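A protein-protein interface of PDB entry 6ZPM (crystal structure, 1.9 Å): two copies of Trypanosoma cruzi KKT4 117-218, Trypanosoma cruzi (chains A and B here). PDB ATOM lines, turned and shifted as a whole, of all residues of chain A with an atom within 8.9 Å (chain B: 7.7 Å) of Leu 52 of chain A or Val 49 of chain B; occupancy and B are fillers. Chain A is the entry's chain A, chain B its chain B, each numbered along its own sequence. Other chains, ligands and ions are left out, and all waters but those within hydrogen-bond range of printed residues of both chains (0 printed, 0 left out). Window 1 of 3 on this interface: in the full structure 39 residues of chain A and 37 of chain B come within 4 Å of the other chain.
Thr 42 of chain A touches Thr 42 of chain B. Thr 42 of chain A touches Leu 45 of chain B. Leu 45 of chain A touches Thr 42 of chain B. Met 46 of chain B touches Leu 45 of chain A (CG to CD1, 3.7 Å). CG1 of Val 49 of chain B touches CD of Arg 48 of chain A, at 3.8 Å. Val 49 of chain A touches Val 49 of chain B. Leu 52 of chain B touches Val 49 of chain A. CD1 of Leu 52 of chain A touches CG2 of Val 53 of chain B (3.7 Å). CD1 of Leu 52 of chain B touches CG2 of Val 53 of chain A, 3.8 Å away. Val 56 of chain A touches Val 56 of chain B.
Leu 45 of chain A touches its own counterpart, Leu 45 of chain B. Leu 45 of chain A touches Met 46 of chain B, but with the chains exchanged Met 46 of chain A does not touch Leu 45 of chain B (4.4 Å). Val 49 of chain A touches its own counterpart, Val 49 of chain B. Val 56 of chain A touches Gln 59 of chain B, and with the chains exchanged Gln 59 of chain A touches Val 56 of chain B. Of the 16 pairs that touch across the chains among the printed residues, 14 have their exchanged pair printed and touching as well.
The backbone carbonyl oxygen (O) of Val 56 of chain A lies close to the side-chain amide oxygen (OE1) of Gln 59 of chain B (3.3 Å). O of Val 56 of chain B lies within hydrogen-bond range of NE2 of Gln 59 of chain A, 3.4 Å away. OE1 of Gln 59 of chain A sits close to OE1 of Gln 59 of chain B, 2.8 Å away.
Leu 52 of chain A touches just these residues of chain B: Val 49 (3.7 Å), Leu 52 (3.6 Å) and Val 53 (3.7 Å). Val 49 of chain B touches just these residues of chain A: Arg 48 (3.8 Å), Val 49 (3.6 Å) and Leu 52 (3.7 Å). Printed residues of chain A within 4 Å of Val 56 of chain B: Val 56 (3.9 Å) and Gln 59 (3.4 Å). Printed residues of chain A within 4 Å of Gln 59 of chain B: Val 56 (3.3 Å) and Gln 59 (2.8 Å). Printed residues of chain A within 4 Å of Met 46 of chain B: Leu 45. The nearest residue of chain B that does not touch Leu 52 of chain A is Val 56 of chain B (4.1 Å).
Printed residues of chain B that touch a printed residue of chain A: Thr 42, Leu 45, Met 46, Val 49, Leu 52, Val 53, Val 56 and Gln 59. Printed residues of chain A that touch a printed residue of chain B: Thr 42, Leu 45, Arg 48, Val 49, Leu 52, Val 53, Val 56 and Gln 59. Hydrophobic or aromatic side chains of chain A that line the printed part of chain B: Leu 45, Val 49, Leu 52, Val 53 and Val 56. Among the printed residues, no Asp or Glu carboxylate lies within 4 Å of a Lys or Arg side-chain nitrogen of the other chain.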
ATOM      1  N   GLU A  41       8.515  32.038  18.390  1.00  0.00           N
ATOM      2  CA  GLU A  41       9.730  31.967  17.584  1.00  0.00           C
ATOM      3  C   GLU A  41      10.942  31.613  18.435  1.00  0.00           C
ATOM      4  O   GLU A  41      11.845  30.914  17.966  1.00  0.00           O
ATOM      5  CB  GLU A  41       9.957  33.291  16.856  1.00  0.00           C
ATOM      6  N   THR A  42      10.974  32.077  19.687  1.00  0.00           N
ATOM      7  CA  THR A  42      12.087  31.755  20.575  1.00  0.00           C
ATOM      8  C   THR A  42      12.177  30.255  20.836  1.00  0.00           C
ATOM      9  O   THR A  42      13.269  29.675  20.792  1.00  0.00           O
ATOM     10  CB  THR A  42      11.945  32.521  21.892  1.00  0.00           C
ATOM     11  OG1 THR A  42      12.016  33.930  21.638  1.00  0.00           O
ATOM     12  CG2 THR A  42      13.045  32.132  22.864  1.00  0.00           C
ATOM     13  N   ARG A  44      10.825  27.908  18.942  1.00  0.00           N
ATOM     14  CA  ARG A  44      11.080  27.261  17.659  1.00  0.00           C
ATOM     15  C   ARG A  44      12.560  27.309  17.308  1.00  0.00           C
ATOM     16  O   ARG A  44      13.134  26.306  16.870  1.00  0.00           O
ATOM     17  CB  ARG A  44      10.248  27.924  16.561  1.00  0.00           C
ATOM     18  N   LEU A  45      13.196  28.467  17.504  1.00  0.00           N
ATOM     19  CA  LEU A  45      14.626  28.576  17.242  1.00  0.00           C
ATOM     20  C   LEU A  45      15.435  27.751  18.235  1.00  0.00           C
ATOM     21  O   LEU A  45      16.402  27.083  17.851  1.00  0.00           O
ATOM     22  CB  LEU A  45      15.056  30.041  17.279  1.00  0.00           C
ATOM     23  CG  LEU A  45      14.512  30.917  16.151  1.00  0.00           C
ATOM     24  CD1 LEU A  45      14.745  32.387  16.462  1.00  0.00           C
ATOM     25  CD2 LEU A  45      15.150  30.538  14.822  1.00  0.00           C
ATOM     26  N   MET A  46      15.059  27.786  19.515  1.00  0.00           N
ATOM     27  CA  MET A  46      15.750  26.971  20.511  1.00  0.00           C
ATOM     28  C   MET A  46      15.679  25.491  20.155  1.00  0.00           C
ATOM     29  O   MET A  46      16.668  24.760  20.302  1.00  0.00           O
ATOM     30  CB  MET A  46      15.150  27.219  21.894  1.00  0.00           C
ATOM     31  CG  MET A  46      16.072  26.868  23.052  1.00  0.00           C
ATOM     32  SD  MET A  46      15.674  27.788  24.556  1.00  0.00           S
ATOM     33  CE  MET A  46      14.584  29.052  23.915  1.00  0.00           C
ATOM     34  N   ARG A  47      14.518  25.035  19.677  1.00  0.00           N
ATOM     35  CA  ARG A  47      14.376  23.638  19.279  1.00  0.00           C
ATOM     36  C   ARG A  47      15.304  23.296  18.118  1.00  0.00           C
ATOM     37  O   ARG A  47      15.842  22.184  18.051  1.00  0.00           O
ATOM     38  CB  ARG A  47      12.921  23.347  18.910  1.00  0.00           C
ATOM     39  N   ARG A  48      15.508  24.238  17.196  1.00  0.00           N
ATOM     40  CA  ARG A  48      16.385  23.959  16.065  1.00  0.00           C
ATOM     41  C   ARG A  48      17.850  23.956  16.480  1.00  0.00           C
ATOM     42  O   ARG A  48      18.642  23.176  15.934  1.00  0.00           O
ATOM     43  CB  ARG A  48      16.151  24.968  14.941  1.00  0.00           C
ATOM     44  CG  ARG A  48      16.309  24.351  13.560  1.00  0.00           C
ATOM     45  CD  ARG A  48      16.838  25.347  12.541  1.00  0.00           C
ATOM     46  NE  ARG A  48      17.432  24.668  11.392  1.00  0.00           N
ATOM     47  CZ  ARG A  48      16.818  24.492  10.225  1.00  0.00           C
ATOM     48  NH1 ARG A  48      15.585  24.945  10.046  1.00  0.00           N
ATOM     49  NH2 ARG A  48      17.439  23.861   9.238  1.00  0.00           N
ATOM     50  N   VAL A  49      18.227  24.808  17.436  1.00  0.00           N
ATOM     51  CA  VAL A  49      19.598  24.800  17.943  1.00  0.00           C
ATOM     52  C   VAL A  49      19.935  23.434  18.529  1.00  0.00           C
ATOM     53  O   VAL A  49      20.998  22.864  18.251  1.00  0.00           O
ATOM     54  CB  VAL A  49      19.797  25.923  18.978  1.00  0.00           C
ATOM     55  CG1 VAL A  49      20.966  25.601  19.902  1.00  0.00           C
ATOM     56  CG2 VAL A  49      20.015  27.259  18.286  1.00  0.00           C
ATOM     57  N   GLU A  50      19.025  22.886  19.338  1.00  0.00           N
ATOM     58  CA  GLU A  50      19.253  21.575  19.938  1.00  0.00           C
ATOM     59  C   GLU A  50      19.327  20.487  18.875  1.00  0.00           C
ATOM     60  O   GLU A  50      20.098  19.528  19.009  1.00  0.00           O
ATOM     61  CB  GLU A  50      18.148  21.263  20.947  1.00  0.00           C
ATOM     62  CG  GLU A  50      18.599  21.298  22.395  1.00  0.00           C
ATOM     63  CD  GLU A  50      19.619  20.224  22.712  1.00  0.00           C
ATOM     64  OE1 GLU A  50      19.469  19.091  22.210  1.00  0.00           O
ATOM     65  OE2 GLU A  50      20.578  20.519  23.456  1.00  0.00           O
ATOM     66  N   GLN A  51      18.524  20.611  17.817  1.00  0.00           N
ATOM     67  CA  GLN A  51      18.587  19.649  16.721  1.00  0.00           C
ATOM     68  C   GLN A  51      19.945  19.701  16.036  1.00  0.00           C
ATOM     69  O   GLN A  51      20.620  18.675  15.882  1.00  0.00           O
ATOM     70  CB  GLN A  51      17.458  19.924  15.722  1.00  0.00           C
ATOM     71  CG  GLN A  51      17.013  18.727  14.876  1.00  0.00           C
ATOM     72  CD  GLN A  51      18.164  18.004  14.195  1.00  0.00           C
ATOM     73  OE1 GLN A  51      18.901  18.594  13.403  1.00  0.00           O
ATOM     74  NE2 GLN A  51      18.320  16.716  14.497  1.00  0.00           N
ATOM     75  N   LEU A  52      20.365  20.897  15.621  1.00  0.00           N
ATOM     76  CA  LEU A  52      21.610  21.024  14.877  1.00  0.00           C
ATOM     77  C   LEU A  52      22.812  20.606  15.714  1.00  0.00           C
ATOM     78  O   LEU A  52      23.768  20.028  15.182  1.00  0.00           O
ATOM     79  CB  LEU A  52      21.766  22.459  14.374  1.00  0.00           C
ATOM     80  CG  LEU A  52      20.694  22.901  13.373  1.00  0.00           C
ATOM     81  CD1 LEU A  52      20.792  24.392  13.074  1.00  0.00           C
ATOM     82  CD2 LEU A  52      20.793  22.087  12.093  1.00  0.00           C
ATOM     83  N   VAL A  53      22.786  20.878  17.020  1.00  0.00           N
ATOM     84  CA  VAL A  53      23.870  20.422  17.885  1.00  0.00           C
ATOM     85  C   VAL A  53      23.911  18.898  17.926  1.00  0.00           C
ATOM     86  O   VAL A  53      24.988  18.289  17.871  1.00  0.00           O
ATOM     87  CB  VAL A  53      23.719  21.033  19.291  1.00  0.00           C
ATOM     88  CG1 VAL A  53      24.608  20.313  20.292  1.00  0.00           C
ATOM     89  CG2 VAL A  53      24.050  22.521  19.260  1.00  0.00           C
ATOM     90  N   SER A  54      22.742  18.257  18.004  1.00  0.00           N
ATOM     91  CA  SER A  54      22.696  16.797  17.975  1.00  0.00           C
ATOM     92  C   SER A  54      23.183  16.254  16.637  1.00  0.00           C
ATOM     93  O   SER A  54      23.883  15.233  16.589  1.00  0.00           O
ATOM     94  CB  SER A  54      21.276  16.313  18.265  1.00  0.00           C
ATOM     95  OG  SER A  54      20.494  16.287  17.082  1.00  0.00           O
ATOM     96  N   ALA A  55      22.825  16.923  15.537  1.00  0.00           N
ATOM     97  CA  ALA A  55      23.297  16.498  14.224  1.00  0.00           C
ATOM     98  C   ALA A  55      24.811  16.610  14.122  1.00  0.00           C
ATOM     99  O   ALA A  55      25.463  15.768  13.494  1.00  0.00           O
ATOM    100  CB  ALA A  55      22.627  17.325  13.127  1.00  0.00           C
ATOM    101  N   VAL A  56      25.387  17.643  14.738  1.00  0.00           N
ATOM    102  CA  VAL A  56      26.835  17.825  14.704  1.00  0.00           C
ATOM    103  C   VAL A  56      27.529  16.669  15.414  1.00  0.00           C
ATOM    104  O   VAL A  56      28.466  16.064  14.882  1.00  0.00           O
ATOM    105  CB  VAL A  56      27.219  19.185  15.317  1.00  0.00           C
ATOM    106  CG1 VAL A  56      28.681  19.191  15.734  1.00  0.00           C
ATOM    107  CG2 VAL A  56      26.942  20.307  14.324  1.00  0.00           C
ATOM    108  N   GLU A  57      27.066  16.336  16.622  1.00  0.00           N
ATOM    109  CA  GLU A  57      27.673  15.245  17.378  1.00  0.00           C
ATOM    110  C   GLU A  57      27.478  13.903  16.686  1.00  0.00           C
ATOM    111  O   GLU A  57      28.326  13.010  16.811  1.00  0.00           O
ATOM    112  CB  GLU A  57      27.093  15.202  18.792  1.00  0.00           C
ATOM    113  N   GLY A  58      26.371  13.735  15.961  1.00  0.00           N
ATOM    114  CA  GLY A  58      26.181  12.511  15.201  1.00  0.00           C
ATOM    115  C   GLY A  58      27.149  12.392  14.039  1.00  0.00           C
ATOM    116  O   GLY A  58      27.671  11.308  13.760  1.00  0.00           O
ATOM    117  N   GLN A  59      27.407  13.504  13.347  1.00  0.00           N
ATOM    118  CA  GLN A  59      28.345  13.477  12.230  1.00  0.00           C
ATOM    119  C   GLN A  59      29.780  13.287  12.702  1.00  0.00           C
ATOM    120  O   GLN A  59      30.590  12.683  11.990  1.00  0.00           O
ATOM    121  CB  GLN A  59      28.231  14.762  11.413  1.00  0.00           C
ATOM    122  CG  GLN A  59      26.971  14.865  10.573  1.00  0.00           C
ATOM    123  CD  GLN A  59      26.883  16.189   9.838  1.00  0.00           C
ATOM    124  OE1 GLN A  59      27.170  17.243  10.403  1.00  0.00           O
ATOM    125  NE2 GLN A  59      26.484  16.142   8.573  1.00  0.00           N
ATOM    126  N   THR B  42      16.077  36.330  19.989  1.00  0.00           N
ATOM    127  CA  THR B  42      15.792  35.758  18.673  1.00  0.00           C
ATOM    128  C   THR B  42      16.946  35.993  17.708  1.00  0.00           C
ATOM    129  O   THR B  42      17.370  35.076  16.995  1.00  0.00           O
ATOM    130  CB  THR B  42      14.497  36.338  18.100  1.00  0.00           C
ATOM    131  OG1 THR B  42      14.516  37.768  18.203  1.00  0.00           O
ATOM    132  CG2 THR B  42      13.288  35.791  18.844  1.00  0.00           C
ATOM    133  N   THR B  43      17.467  37.222  17.668  1.00  0.00           N
ATOM    134  CA  THR B  43      18.604  37.510  16.798  1.00  0.00           C
ATOM    135  C   THR B  43      19.816  36.667  17.181  1.00  0.00           C
ATOM    136  O   THR B  43      20.521  36.149  16.307  1.00  0.00           O
ATOM    137  CB  THR B  43      18.943  39.000  16.848  1.00  0.00           C
ATOM    138  OG1 THR B  43      19.034  39.426  18.213  1.00  0.00           O
ATOM    139  CG2 THR B  43      17.868  39.813  16.139  1.00  0.00           C
ATOM    140  N   ARG B  44      20.063  36.508  18.484  1.00  0.00           N
ATOM    141  CA  ARG B  44      21.159  35.654  18.933  1.00  0.00           C
ATOM    142  C   ARG B  44      20.914  34.197  18.553  1.00  0.00           C
ATOM    143  O   ARG B  44      21.853  33.474  18.194  1.00  0.00           O
ATOM    144  CB  ARG B  44      21.342  35.800  20.444  1.00  0.00           C
ATOM    145  CG  ARG B  44      22.414  34.905  21.033  1.00  0.00           C
ATOM    146  CD  ARG B  44      22.486  35.058  22.542  1.00  0.00           C
ATOM    147  NE  ARG B  44      22.920  33.822  23.186  1.00  0.00           N
ATOM    148  CZ  ARG B  44      22.102  32.827  23.509  1.00  0.00           C
ATOM    149  NH1 ARG B  44      20.805  32.928  23.251  1.00  0.00           N
ATOM    150  NH2 ARG B  44      22.575  31.732  24.089  1.00  0.00           N
ATOM    151  N   LEU B  45      19.654  33.750  18.619  1.00  0.00           N
ATOM    152  CA  LEU B  45      19.308  32.394  18.192  1.00  0.00           C
ATOM    153  C   LEU B  45      19.487  32.196  16.693  1.00  0.00           C
ATOM    154  O   LEU B  45      20.045  31.181  16.266  1.00  0.00           O
ATOM    155  CB  LEU B  45      17.879  32.054  18.606  1.00  0.00           C
ATOM    156  CG  LEU B  45      17.753  31.942  20.120  1.00  0.00           C
ATOM    157  CD1 LEU B  45      16.296  31.837  20.531  1.00  0.00           C
ATOM    158  CD2 LEU B  45      18.584  30.740  20.649  1.00  0.00           C
ATOM    159  N   MET B  46      18.997  33.133  15.878  1.00  0.00           N
ATOM    160  CA  MET B  46      19.116  32.979  14.431  1.00  0.00           C
ATOM    161  C   MET B  46      20.573  32.942  13.991  1.00  0.00           C
ATOM    162  O   MET B  46      20.908  32.290  12.994  1.00  0.00           O
ATOM    163  CB  MET B  46      18.373  34.114  13.727  1.00  0.00           C
ATOM    164  CG  MET B  46      16.876  34.115  13.986  1.00  0.00           C
ATOM    165  SD  MET B  46      16.107  35.669  13.501  1.00  0.00           S
ATOM    166  CE  MET B  46      16.713  35.819  11.823  1.00  0.00           C
ATOM    167  N   ARG B  47      21.453  33.621  14.729  1.00  0.00           N
ATOM    168  CA  ARG B  47      22.870  33.608  14.391  1.00  0.00           C
ATOM    169  C   ARG B  47      23.482  32.238  14.657  1.00  0.00           C
ATOM    170  O   ARG B  47      24.161  31.674  13.792  1.00  0.00           O
ATOM    171  CB  ARG B  47      23.606  34.696  15.174  1.00  0.00           C
ATOM    172  N   ARG B  48      23.246  31.679  15.848  1.00  0.00           N
ATOM    173  CA  ARG B  48      23.824  30.376  16.155  1.00  0.00           C
ATOM    174  C   ARG B  48      23.214  29.274  15.297  1.00  0.00           C
ATOM    175  O   ARG B  48      23.904  28.310  14.952  1.00  0.00           O
ATOM    176  CB  ARG B  48      23.664  30.040  17.637  1.00  0.00           C
ATOM    177  CG  ARG B  48      24.479  28.818  18.036  1.00  0.00           C
ATOM    178  CD  ARG B  48      24.292  28.419  19.486  1.00  0.00           C
ATOM    179  NE  ARG B  48      25.064  27.217  19.802  1.00  0.00           N
ATOM    180  CZ  ARG B  48      25.196  26.708  21.023  1.00  0.00           C
ATOM    181  NH1 ARG B  48      24.606  27.293  22.057  1.00  0.00           N
ATOM    182  NH2 ARG B  48      25.918  25.611  21.208  1.00  0.00           N
ATOM    183  N   VAL B  49      21.931  29.393  14.944  1.00  0.00           N
ATOM    184  CA  VAL B  49      21.341  28.456  13.990  1.00  0.00           C
ATOM    185  C   VAL B  49      22.087  28.523  12.663  1.00  0.00           C
ATOM    186  O   VAL B  49      22.432  27.495  12.067  1.00  0.00           O
ATOM    187  CB  VAL B  49      19.840  28.746  13.806  1.00  0.00           C
ATOM    188  CG1 VAL B  49      19.345  28.190  12.475  1.00  0.00           C
ATOM    189  CG2 VAL B  49      19.038  28.170  14.962  1.00  0.00           C
ATOM    190  N   GLU B  50      22.362  29.740  12.192  1.00  0.00           N
ATOM    191  CA  GLU B  50      23.059  29.902  10.921  1.00  0.00           C
ATOM    192  C   GLU B  50      24.469  29.326  10.984  1.00  0.00           C
ATOM    193  O   GLU B  50      24.938  28.705  10.022  1.00  0.00           O
ATOM    194  CB  GLU B  50      23.093  31.379  10.540  1.00  0.00           C
ATOM    195  CG  GLU B  50      22.765  31.626   9.089  1.00  0.00           C
ATOM    196  CD  GLU B  50      21.605  30.780   8.606  1.00  0.00           C
ATOM    197  OE1 GLU B  50      21.832  29.881   7.768  1.00  0.00           O
ATOM    198  OE2 GLU B  50      20.467  31.013   9.063  1.00  0.00           O
ATOM    199  N   GLN B  51      25.158  29.520  12.110  1.00  0.00           N
ATOM    200  CA  GLN B  51      26.483  28.934  12.278  1.00  0.00           C
ATOM    201  C   GLN B  51      26.412  27.413  12.309  1.00  0.00           C
ATOM    202  O   GLN B  51      27.280  26.730  11.750  1.00  0.00           O
ATOM    203  CB  GLN B  51      27.131  29.473  13.553  1.00  0.00           C
ATOM    204  CG  GLN B  51      28.343  28.687  14.019  1.00  0.00           C
ATOM    205  CD  GLN B  51      28.770  29.055  15.425  1.00  0.00           C
ATOM    206  OE1 GLN B  51      28.024  28.856  16.383  1.00  0.00           O
ATOM    207  NE2 GLN B  51      29.978  29.591  15.556  1.00  0.00           N
ATOM    208  N   LEU B  52      25.377  26.864  12.947  1.00  0.00           N
ATOM    209  CA  LEU B  52      25.249  25.415  13.036  1.00  0.00           C
ATOM    210  C   LEU B  52      24.915  24.792  11.687  1.00  0.00           C
ATOM    211  O   LEU B  52      25.377  23.684  11.390  1.00  0.00           O
ATOM    212  CB  LEU B  52      24.191  25.051  14.076  1.00  0.00           C
ATOM    213  CG  LEU B  52      24.620  25.218  15.535  1.00  0.00           C
ATOM    214  CD1 LEU B  52      23.432  25.059  16.472  1.00  0.00           C
ATOM    215  CD2 LEU B  52      25.723  24.229  15.885  1.00  0.00           C
ATOM    216  N   VAL B  53      24.122  25.478  10.859  1.00  0.00           N
ATOM    217  CA  VAL B  53      23.824  24.957   9.527  1.00  0.00           C
ATOM    218  C   VAL B  53      25.090  24.909   8.681  1.00  0.00           C
ATOM    219  O   VAL B  53      25.342  23.929   7.967  1.00  0.00           O
ATOM    220  CB  VAL B  53      22.719  25.794   8.858  1.00  0.00           C
ATOM    221  CG1 VAL B  53      22.592  25.434   7.384  1.00  0.00           C
ATOM    222  CG2 VAL B  53      21.394  25.580   9.571  1.00  0.00           C
ATOM    223  N   SER B  54      25.910  25.961   8.753  1.00  0.00           N
ATOM    224  CA  SER B  54      27.204  25.937   8.081  1.00  0.00           C
ATOM    225  C   SER B  54      28.100  24.840   8.638  1.00  0.00           C
ATOM    226  O   SER B  54      28.901  24.258   7.898  1.00  0.00           O
ATOM    227  CB  SER B  54      27.891  27.295   8.211  1.00  0.00           C
ATOM    228  OG  SER B  54      28.391  27.483   9.526  1.00  0.00           O
ATOM    229  N   ALA B  55      27.980  24.543   9.935  1.00  0.00           N
ATOM    230  CA  ALA B  55      28.781  23.479  10.532  1.00  0.00           C
ATOM    231  C   ALA B  55      28.351  22.111  10.020  1.00  0.00           C
ATOM    232  O   ALA B  55      29.193  21.284   9.645  1.00  0.00           O
ATOM    233  CB  ALA B  55      28.683  23.538  12.057  1.00  0.00           C
ATOM    234  N   VAL B  56      27.041  21.851  10.000  1.00  0.00           N
ATOM    235  CA  VAL B  56      26.545  20.562   9.521  1.00  0.00           C
ATOM    236  C   VAL B  56      26.964  20.337   8.072  1.00  0.00           C
ATOM    237  O   VAL B  56      27.446  19.258   7.706  1.00  0.00           O
ATOM    238  CB  VAL B  56      25.017  20.476   9.688  1.00  0.00           C
ATOM    239  CG1 VAL B  56      24.484  19.201   9.047  1.00  0.00           C
ATOM    240  CG2 VAL B  56      24.637  20.532  11.165  1.00  0.00           C
ATOM    241  N   GLN B  59      30.677  19.435   8.006  1.00  0.00           N
ATOM    242  CA  GLN B  59      30.961  18.048   8.365  1.00  0.00           C
ATOM    243  C   GLN B  59      30.510  17.095   7.267  1.00  0.00           C
ATOM    244  O   GLN B  59      31.168  16.078   7.010  1.00  0.00           O
ATOM    245  CB  GLN B  59      30.288  17.694   9.692  1.00  0.00           C
ATOM    246  CG  GLN B  59      31.184  17.844  10.917  1.00  0.00           C
ATOM    247  CD  GLN B  59      30.413  17.739  12.222  1.00  0.00           C
ATOM    248  OE1 GLN B  59      29.201  17.946  12.256  1.00  0.00           O
ATOM    249  NE2 GLN B  59      31.116  17.420  13.305  1.00  0.00           N
